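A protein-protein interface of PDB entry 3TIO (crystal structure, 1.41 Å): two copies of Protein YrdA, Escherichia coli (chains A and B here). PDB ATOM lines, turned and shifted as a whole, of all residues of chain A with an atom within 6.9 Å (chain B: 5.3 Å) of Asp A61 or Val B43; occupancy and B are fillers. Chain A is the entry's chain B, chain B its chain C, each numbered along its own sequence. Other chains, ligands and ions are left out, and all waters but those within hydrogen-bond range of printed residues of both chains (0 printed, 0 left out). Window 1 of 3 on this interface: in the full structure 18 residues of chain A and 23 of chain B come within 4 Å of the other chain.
CB of Ser A23 touches CG2 of Val B25 (3.9 Å).
NH1 of Arg B45 touches CZ3 of Trp A39, 3.5 Å away.
CG of Pro A40 touches CD1 of Ile B27, 3.98 Å away.
Pro A40 touches Val B43.
Leu A41 touches Leu B41.
Val B43 touches Leu A41.
Asp A61 touches Val B43.
OD2 of Asp A61 touches CE of Met B64, at 3.7 Å.
CE1 of His A90 touches NH2 of Arg B45, 3.5 Å away.
CB of Met B64 touches CE of Lys A91 (3.6 Å).
Of the 18 printed residues of chain A, 8 touch a printed residue of chain B.
Of the 10 printed residues of chain B, 6 touch a printed residue of chain A.
Printed residues of chain B that touch a printed residue of chain A: Val B25, Ile B27, Leu B41, Val B43, Arg B45 and Met B64.
Hydrophobic or aromatic side chains of chain B within 4 Å of the printed part of chain A: Val B25, Ile B27, Val B43 and Met B64.
Along chain B the printed residues that touch a printed residue of chain A span positions 25 to 64.
Among the printed residues, Asp or Glu carboxylates within 4 Å of a Lys or Arg side-chain nitrogen of the other chain: Asp A61 with Arg B45.
The backbone carbonyl oxygen (O) of Leu A41 sits close to the backbone NH (N) of Gly A62.
The side-chain hydroxyl (OG) of Ser A24 lies within hydrogen-bond range of the backbone carbonyl oxygen (O) of Trp A39 (2.7 Å).
N of Ile B44 lies within hydrogen-bond range of O of Val B25 (2.9 Å).
OG of Ser A24 lies within hydrogen-bond range of N of Leu A41.
The backbone NH (N) of Val B43 is in hydrogen-bond range of the backbone carbonyl oxygen (O) of Ser B63, at 3.2 Å.
The side-chain hydroxyl of Tyr A167 sits at hydrogen-bond distance from the side-chain amide oxygen of Gln A60, at 2.8 Å.
Leu B41 touches its own counterpart, Leu A41.
Of the 13 pairs that touch across the chains among the printed residues, 1 has its exchanged pair printed and touching as well.
Asp A61 touches just these residues of chain B: Val B43, Arg B45 and Met B64.
Of the printed residues of chain A, Val B43 touches Pro A40, Leu A41 and Asp A61.
Printed residues of chain B within 4 Å of Trp A39: Arg B45.
Printed residues of chain B within 4 Å of His A90: Arg B45 and Met B64.
Of the printed residues of chain B, Pro A40 touches Ile B27 (3.98 Å) and Val B43 (3.9 Å).
Of the printed residues of chain A, Leu B41 touches Leu A41.
Printed residues of chain A within 4 Å of Val B25: Ser A23.
A ring nitrogen (ND1) of His A90 sits at hydrogen-bond distance from the side-chain sulfur (SD) of Met B64.
OD1 of Asp A61 is in salt-bridge range of NH2 of Arg B45 (2.7 Å).
The side-chain hydroxyl (OH) of Tyr A167 sits at hydrogen-bond distance from the guanidinium group (NH2) of Arg B45, at 3.0 Å.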
ATOM      1  N   SER A  23       3.553   4.628   0.890  1.00  0.00           N
ATOM      2  CA  SER A  23       3.351   3.483   0.004  1.00  0.00           C
ATOM      3  C   SER A  23       3.130   3.884  -1.453  1.00  0.00           C
ATOM      4  O   SER A  23       2.958   3.025  -2.316  1.00  0.00           O
ATOM      5  CB  SER A  23       2.152   2.655   0.477  1.00  0.00           C
ATOM      6  OG  SER A  23       0.936   3.343   0.230  1.00  0.00           O
ATOM      7  N   SER A  24       3.147   5.181  -1.735  1.00  0.00           N
ATOM      8  CA  SER A  24       2.910   5.633  -3.093  1.00  0.00           C
ATOM      9  C   SER A  24       4.178   5.885  -3.892  1.00  0.00           C
ATOM     10  O   SER A  24       5.276   5.940  -3.340  1.00  0.00           O
ATOM     11  CB  SER A  24       1.998   6.857  -3.071  1.00  0.00           C
ATOM     12  OG  SER A  24       0.715   6.458  -2.598  1.00  0.00           O
ATOM     13  N   ILE A  38      -1.790  12.866  -1.657  1.00  0.00           N
ATOM     14  CA  ILE A  38      -1.667  11.640  -2.439  1.00  0.00           C
ATOM     15  C   ILE A  38      -1.787  10.494  -1.448  1.00  0.00           C
ATOM     16  O   ILE A  38      -0.908  10.287  -0.612  1.00  0.00           O
ATOM     17  CB  ILE A  38      -0.300  11.562  -3.146  1.00  0.00           C
ATOM     18  CG1 ILE A  38      -0.034  12.857  -3.923  1.00  0.00           C
ATOM     19  CG2 ILE A  38      -0.257  10.335  -4.049  1.00  0.00           C
ATOM     20  CD1 ILE A  38      -1.092  13.214  -4.942  1.00  0.00           C
ATOM     21  N   TRP A  39      -2.872   9.738  -1.558  1.00  0.00           N
ATOM     22  CA  TRP A  39      -3.143   8.657  -0.629  1.00  0.00           C
ATOM     23  C   TRP A  39      -2.442   7.335  -0.947  1.00  0.00           C
ATOM     24  O   TRP A  39      -1.745   7.226  -1.951  1.00  0.00           O
ATOM     25  CB  TRP A  39      -4.666   8.535  -0.480  1.00  0.00           C
ATOM     26  CG  TRP A  39      -5.210   9.806   0.142  1.00  0.00           C
ATOM     27  CD1 TRP A  39      -5.419  11.007  -0.484  1.00  0.00           C
ATOM     28  CD2 TRP A  39      -5.426  10.047   1.540  1.00  0.00           C
ATOM     29  NE1 TRP A  39      -5.739  11.980   0.440  1.00  0.00           N
ATOM     30  CE2 TRP A  39      -5.750  11.416   1.687  1.00  0.00           C
ATOM     31  CE3 TRP A  39      -5.370   9.240   2.684  1.00  0.00           C
ATOM     32  CZ2 TRP A  39      -6.018  11.994   2.934  1.00  0.00           C
ATOM     33  CZ3 TRP A  39      -5.634   9.817   3.923  1.00  0.00           C
ATOM     34  CH2 TRP A  39      -5.954  11.181   4.035  1.00  0.00           C
ATOM     35  N   PRO A  40      -2.596   6.320  -0.080  1.00  0.00           N
ATOM     36  CA  PRO A  40      -1.947   5.018  -0.289  1.00  0.00           C
ATOM     37  C   PRO A  40      -2.046   4.340  -1.650  1.00  0.00           C
ATOM     38  O   PRO A  40      -3.055   4.437  -2.348  1.00  0.00           O
ATOM     39  CB  PRO A  40      -2.549   4.151   0.815  1.00  0.00           C
ATOM     40  CG  PRO A  40      -2.771   5.133   1.918  1.00  0.00           C
ATOM     41  CD  PRO A  40      -3.347   6.327   1.189  1.00  0.00           C
ATOM     42  N   LEU A  41      -0.967   3.648  -2.000  1.00  0.00           N
ATOM     43  CA  LEU A  41      -0.851   2.881  -3.239  1.00  0.00           C
ATOM     44  C   LEU A  41      -1.269   3.593  -4.519  1.00  0.00           C
ATOM     45  O   LEU A  41      -1.991   3.046  -5.362  1.00  0.00           O
ATOM     46  CB  LEU A  41      -1.598   1.551  -3.093  1.00  0.00           C
ATOM     47  CG  LEU A  41      -1.063   0.652  -1.967  1.00  0.00           C
ATOM     48  CD1 LEU A  41      -1.791  -0.687  -1.990  1.00  0.00           C
ATOM     49  CD2 LEU A  41       0.440   0.430  -2.140  1.00  0.00           C
ATOM     50  N   VAL A  42      -0.792   4.823  -4.657  1.00  0.00           N
ATOM     51  CA  VAL A  42      -1.050   5.634  -5.834  1.00  0.00           C
ATOM     52  C   VAL A  42       0.250   5.710  -6.632  1.00  0.00           C
ATOM     53  O   VAL A  42       1.337   5.726  -6.050  1.00  0.00           O
ATOM     54  CB  VAL A  42      -1.453   7.077  -5.441  1.00  0.00           C
ATOM     55  CG1 VAL A  42      -1.445   7.982  -6.663  1.00  0.00           C
ATOM     56  CG2 VAL A  42      -2.825   7.073  -4.792  1.00  0.00           C
ATOM     57  N   ILE A  59      -5.795  12.909  -4.441  1.00  0.00           N
ATOM     58  CA  ILE A  59      -5.671  11.777  -5.355  1.00  0.00           C
ATOM     59  C   ILE A  59      -5.816  10.596  -4.403  1.00  0.00           C
ATOM     60  O   ILE A  59      -4.887  10.245  -3.674  1.00  0.00           O
ATOM     61  CB  ILE A  59      -4.288  11.746  -6.044  1.00  0.00           C
ATOM     62  CG1 ILE A  59      -4.030  13.067  -6.783  1.00  0.00           C
ATOM     63  CG2 ILE A  59      -4.219  10.570  -7.000  1.00  0.00           C
ATOM     64  CD1 ILE A  59      -5.067  13.433  -7.837  1.00  0.00           C
ATOM     65  N   GLN A  60      -6.995   9.987  -4.404  1.00  0.00           N
ATOM     66  CA  GLN A  60      -7.271   8.919  -3.464  1.00  0.00           C
ATOM     67  C   GLN A  60      -6.649   7.551  -3.728  1.00  0.00           C
ATOM     68  O   GLN A  60      -6.176   7.260  -4.831  1.00  0.00           O
ATOM     69  CB  GLN A  60      -8.785   8.836  -3.252  1.00  0.00           C
ATOM     70  CG  GLN A  60      -9.323  10.106  -2.581  1.00  0.00           C
ATOM     71  CD  GLN A  60     -10.826  10.114  -2.449  1.00  0.00           C
ATOM     72  OE1 GLN A  60     -11.407   9.219  -1.837  1.00  0.00           O
ATOM     73  NE2 GLN A  60     -11.468  11.123  -3.026  1.00  0.00           N
ATOM     74  N   ASP A  61      -6.660   6.729  -2.680  1.00  0.00           N
ATOM     75  CA  ASP A  61      -6.054   5.397  -2.669  1.00  0.00           C
ATOM     76  C   ASP A  61      -6.227   4.560  -3.921  1.00  0.00           C
ATOM     77  O   ASP A  61      -7.336   4.399  -4.420  1.00  0.00           O
ATOM     78  CB  ASP A  61      -6.583   4.556  -1.496  1.00  0.00           C
ATOM     79  CG  ASP A  61      -6.858   5.368  -0.244  1.00  0.00           C
ATOM     80  OD1 ASP A  61      -7.605   6.360  -0.327  1.00  0.00           O
ATOM     81  OD2 ASP A  61      -6.350   4.993   0.833  1.00  0.00           O
ATOM     82  N   GLY A  62      -5.114   4.014  -4.408  1.00  0.00           N
ATOM     83  CA  GLY A  62      -5.149   3.136  -5.566  1.00  0.00           C
ATOM     84  C   GLY A  62      -5.276   3.761  -6.939  1.00  0.00           C
ATOM     85  O   GLY A  62      -5.419   3.037  -7.921  1.00  0.00           O
ATOM     86  N   SER A  63      -5.231   5.084  -7.026  1.00  0.00           N
ATOM     87  CA  SER A  63      -5.337   5.748  -8.319  1.00  0.00           C
ATOM     88  C   SER A  63      -4.049   5.571  -9.123  1.00  0.00           C
ATOM     89  O   SER A  63      -2.980   5.319  -8.566  1.00  0.00           O
ATOM     90  CB  SER A  63      -5.636   7.241  -8.135  1.00  0.00           C
ATOM     91  OG  SER A  63      -6.948   7.439  -7.630  1.00  0.00           O
ATOM     92  N   VAL A  88     -10.184  13.275  -6.770  1.00  0.00           N
ATOM     93  CA  VAL A  88      -9.973  12.104  -7.616  1.00  0.00           C
ATOM     94  C   VAL A  88     -10.230  10.896  -6.713  1.00  0.00           C
ATOM     95  O   VAL A  88      -9.467  10.615  -5.786  1.00  0.00           O
ATOM     96  CB  VAL A  88      -8.533  12.071  -8.187  1.00  0.00           C
ATOM     97  CG1 VAL A  88      -8.328  10.811  -9.018  1.00  0.00           C
ATOM     98  CG2 VAL A  88      -8.290  13.302  -9.047  1.00  0.00           C
ATOM     99  N   GLY A  89     -11.330  10.202  -6.983  1.00  0.00           N
ATOM    100  CA  GLY A  89     -11.720   9.061  -6.170  1.00  0.00           C
ATOM    101  C   GLY A  89     -10.762   7.887  -6.126  1.00  0.00           C
ATOM    102  O   GLY A  89      -9.789   7.828  -6.883  1.00  0.00           O
ATOM    103  N   HIS A  90     -11.041   6.948  -5.226  1.00  0.00           N
ATOM    104  CA  HIS A  90     -10.207   5.760  -5.086  1.00  0.00           C
ATOM    105  C   HIS A  90     -10.167   4.996  -6.401  1.00  0.00           C
ATOM    106  O   HIS A  90     -11.163   4.946  -7.130  1.00  0.00           O
ATOM    107  CB  HIS A  90     -10.777   4.794  -4.046  1.00  0.00           C
ATOM    108  CG  HIS A  90     -11.062   5.415  -2.718  1.00  0.00           C
ATOM    109  ND1 HIS A  90     -10.068   5.768  -1.831  1.00  0.00           N
ATOM    110  CD2 HIS A  90     -12.235   5.708  -2.110  1.00  0.00           C
ATOM    111  CE1 HIS A  90     -10.617   6.250  -0.730  1.00  0.00           C
ATOM    112  NE2 HIS A  90     -11.930   6.224  -0.875  1.00  0.00           N
ATOM    113  N   LYS A  91      -9.016   4.397  -6.685  1.00  0.00           N
ATOM    114  CA  LYS A  91      -8.839   3.572  -7.876  1.00  0.00           C
ATOM    115  C   LYS A  91      -9.155   4.225  -9.209  1.00  0.00           C
ATOM    116  O   LYS A  91      -9.515   3.534 -10.160  1.00  0.00           O
ATOM    117  CB  LYS A  91      -9.686   2.303  -7.750  1.00  0.00           C
ATOM    118  CG  LYS A  91      -9.138   1.265  -6.790  1.00  0.00           C
ATOM    119  CD  LYS A  91      -9.962  -0.015  -6.876  1.00  0.00           C
ATOM    120  CE  LYS A  91      -9.268  -1.168  -6.179  1.00  0.00           C
ATOM    121  NZ  LYS A  91      -7.941  -1.459  -6.791  1.00  0.00           N
ATOM    122  N   VAL A  92      -9.030   5.541  -9.296  1.00  0.00           N
ATOM    123  CA  VAL A  92      -9.303   6.210 -10.558  1.00  0.00           C
ATOM    124  C   VAL A  92      -8.082   6.134 -11.479  1.00  0.00           C
ATOM    125  O   VAL A  92      -6.935   6.227 -11.032  1.00  0.00           O
ATOM    126  CB  VAL A  92      -9.694   7.681 -10.322  1.00  0.00           C
ATOM    127  CG1 VAL A  92      -9.608   8.474 -11.621  1.00  0.00           C
ATOM    128  CG2 VAL A  92     -11.119   7.745  -9.779  1.00  0.00           C
ATOM    129  N   TYR A 167     -11.025  16.783   2.466  1.00  0.00           N
ATOM    130  CA  TYR A 167      -9.805  16.026   2.241  1.00  0.00           C
ATOM    131  C   TYR A 167      -8.538  16.798   2.582  1.00  0.00           C
ATOM    132  O   TYR A 167      -7.515  16.192   2.898  1.00  0.00           O
ATOM    133  CB  TYR A 167      -9.748  15.488   0.809  1.00  0.00           C
ATOM    134  CG  TYR A 167      -9.955  13.989   0.766  1.00  0.00           C
ATOM    135  CD1 TYR A 167     -11.140  13.437   0.282  1.00  0.00           C
ATOM    136  CD2 TYR A 167      -8.981  13.124   1.261  1.00  0.00           C
ATOM    137  CE1 TYR A 167     -11.348  12.052   0.296  1.00  0.00           C
ATOM    138  CE2 TYR A 167      -9.175  11.743   1.278  1.00  0.00           C
ATOM    139  CZ  TYR A 167     -10.360  11.214   0.794  1.00  0.00           C
ATOM    140  OH  TYR A 167     -10.546   9.845   0.800  1.00  0.00           O
ATOM    141  N   VAL B  25      -1.384  -2.238   3.127  1.00  0.00           N
ATOM    142  CA  VAL B  25      -1.502  -1.113   4.044  1.00  0.00           C
ATOM    143  C   VAL B  25      -2.817  -1.150   4.811  1.00  0.00           C
ATOM    144  O   VAL B  25      -3.887  -1.050   4.215  1.00  0.00           O
ATOM    145  CB  VAL B  25      -1.421   0.204   3.240  1.00  0.00           C
ATOM    146  CG1 VAL B  25      -1.398   1.400   4.170  1.00  0.00           C
ATOM    147  CG2 VAL B  25      -0.184   0.185   2.347  1.00  0.00           C
ATOM    148  N   ILE B  27      -4.739   0.759   7.833  1.00  0.00           N
ATOM    149  CA  ILE B  27      -4.741   1.963   8.656  1.00  0.00           C
ATOM    150  C   ILE B  27      -5.963   2.171   9.537  1.00  0.00           C
ATOM    151  O   ILE B  27      -7.098   2.015   9.092  1.00  0.00           O
ATOM    152  CB  ILE B  27      -4.623   3.212   7.752  1.00  0.00           C
ATOM    153  CG1 ILE B  27      -3.377   3.101   6.873  1.00  0.00           C
ATOM    154  CG2 ILE B  27      -4.612   4.482   8.599  1.00  0.00           C
ATOM    155  CD1 ILE B  27      -3.364   4.084   5.713  1.00  0.00           C
ATOM    156  N   LEU B  41      -0.745  -5.762  -2.116  1.00  0.00           N
ATOM    157  CA  LEU B  41      -1.175  -4.433  -2.536  1.00  0.00           C
ATOM    158  C   LEU B  41      -2.636  -4.090  -2.259  1.00  0.00           C
ATOM    159  O   LEU B  41      -3.354  -3.571  -3.116  1.00  0.00           O
ATOM    160  CB  LEU B  41      -0.836  -4.229  -4.018  1.00  0.00           C
ATOM    161  CG  LEU B  41       0.664  -4.324  -4.343  1.00  0.00           C
ATOM    162  CD1 LEU B  41       0.896  -3.973  -5.801  1.00  0.00           C
ATOM    163  CD2 LEU B  41       1.467  -3.381  -3.451  1.00  0.00           C
ATOM    164  N   VAL B  42      -3.058  -4.385  -1.038  1.00  0.00           N
ATOM    165  CA  VAL B  42      -4.405  -4.082  -0.584  1.00  0.00           C
ATOM    166  C   VAL B  42      -4.313  -2.898   0.377  1.00  0.00           C
ATOM    167  O   VAL B  42      -3.336  -2.772   1.117  1.00  0.00           O
ATOM    168  CB  VAL B  42      -5.015  -5.269   0.199  1.00  0.00           C
ATOM    169  CG1 VAL B  42      -6.266  -4.822   0.946  1.00  0.00           C
ATOM    170  CG2 VAL B  42      -5.351  -6.396  -0.749  1.00  0.00           C
ATOM    171  N   VAL B  43      -5.314  -2.024   0.350  1.00  0.00           N
ATOM    172  CA  VAL B  43      -5.370  -0.901   1.274  1.00  0.00           C
ATOM    173  C   VAL B  43      -6.691  -1.000   2.025  1.00  0.00           C
ATOM    174  O   VAL B  43      -7.747  -1.153   1.409  1.00  0.00           O
ATOM    175  CB  VAL B  43      -5.352   0.482   0.569  1.00  0.00           C
ATOM    176  CG1 VAL B  43      -5.448   1.600   1.620  1.00  0.00           C
ATOM    177  CG2 VAL B  43      -4.095   0.641  -0.247  1.00  0.00           C
ATOM    178  N   ILE B  44      -6.629  -0.947   3.349  1.00  0.00           N
ATOM    179  CA  ILE B  44      -7.828  -0.965   4.178  1.00  0.00           C
ATOM    180  C   ILE B  44      -7.640   0.245   5.076  1.00  0.00           C
ATOM    181  O   ILE B  44      -6.670   0.320   5.827  1.00  0.00           O
ATOM    182  CB  ILE B  44      -7.940  -2.236   5.045  1.00  0.00           C
ATOM    183  CG1 ILE B  44      -7.830  -3.487   4.166  1.00  0.00           C
ATOM    184  CG2 ILE B  44      -9.282  -2.240   5.779  1.00  0.00           C
ATOM    185  CD1 ILE B  44      -7.911  -4.799   4.938  1.00  0.00           C
ATOM    186  N   ARG B  45      -8.553   1.200   4.976  1.00  0.00           N
ATOM    187  CA  ARG B  45      -8.461   2.431   5.747  1.00  0.00           C
ATOM    188  C   ARG B  45      -9.713   2.654   6.584  1.00  0.00           C
ATOM    189  O   ARG B  45     -10.801   2.833   6.052  1.00  0.00           O
ATOM    190  CB  ARG B  45      -8.224   3.605   4.780  1.00  0.00           C
ATOM    191  CG  ARG B  45      -8.056   4.980   5.427  1.00  0.00           C
ATOM    192  CD  ARG B  45      -7.104   5.868   4.612  1.00  0.00           C
ATOM    193  NE  ARG B  45      -7.598   6.264   3.288  1.00  0.00           N
ATOM    194  CZ  ARG B  45      -8.341   7.342   3.047  1.00  0.00           C
ATOM    195  NH1 ARG B  45      -8.697   8.148   4.038  1.00  0.00           N
ATOM    196  NH2 ARG B  45      -8.695   7.645   1.803  1.00  0.00           N
ATOM    197  N   SER B  63      -7.232  -5.037  -3.774  1.00  0.00           N
ATOM    198  CA  SER B  63      -8.503  -4.495  -3.314  1.00  0.00           C
ATOM    199  C   SER B  63      -8.290  -3.203  -2.533  1.00  0.00           C
ATOM    200  O   SER B  63      -7.203  -2.950  -2.007  1.00  0.00           O
ATOM    201  CB  SER B  63      -9.238  -5.520  -2.446  1.00  0.00           C
ATOM    202  OG  SER B  63      -9.706  -6.605  -3.233  1.00  0.00           O
ATOM    203  N   MET B  64      -9.334  -2.383  -2.472  1.00  0.00           N
ATOM    204  CA  MET B  64      -9.285  -1.108  -1.763  1.00  0.00           C
ATOM    205  C   MET B  64     -10.549  -1.039  -0.918  1.00  0.00           C
ATOM    206  O   MET B  64     -11.660  -1.064  -1.449  1.00  0.00           O
ATOM    207  CB  MET B  64      -9.247   0.048  -2.774  1.00  0.00           C
ATOM    208  CG  MET B  64      -8.679   1.373  -2.247  1.00  0.00           C
ATOM    209  SD  MET B  64      -9.705   2.226  -1.031  1.00  0.00           S
ATOM    210  CE  MET B  64      -8.670   2.169   0.430  1.00  0.00           C
ATOM    211  N   LEU B  65     -10.372  -0.972   0.397  1.00  0.00           N
ATOM    212  CA  LEU B  65     -11.487  -0.925   1.333  1.00  0.00           C
ATOM    213  C   LEU B  65     -11.467   0.359   2.143  1.00  0.00           C
ATOM    214  O   LEU B  65     -10.461   0.679   2.777  1.00  0.00           O
ATOM    215  CB  LEU B  65     -11.417  -2.120   2.288  1.00  0.00           C
ATOM    216  CG  LEU B  65     -11.909  -3.486   1.803  1.00  0.00           C
ATOM    217  CD1 LEU B  65     -11.209  -3.882   0.519  1.00  0.00           C
ATOM    218  CD2 LEU B  65     -11.649  -4.521   2.891  1.00  0.00           C
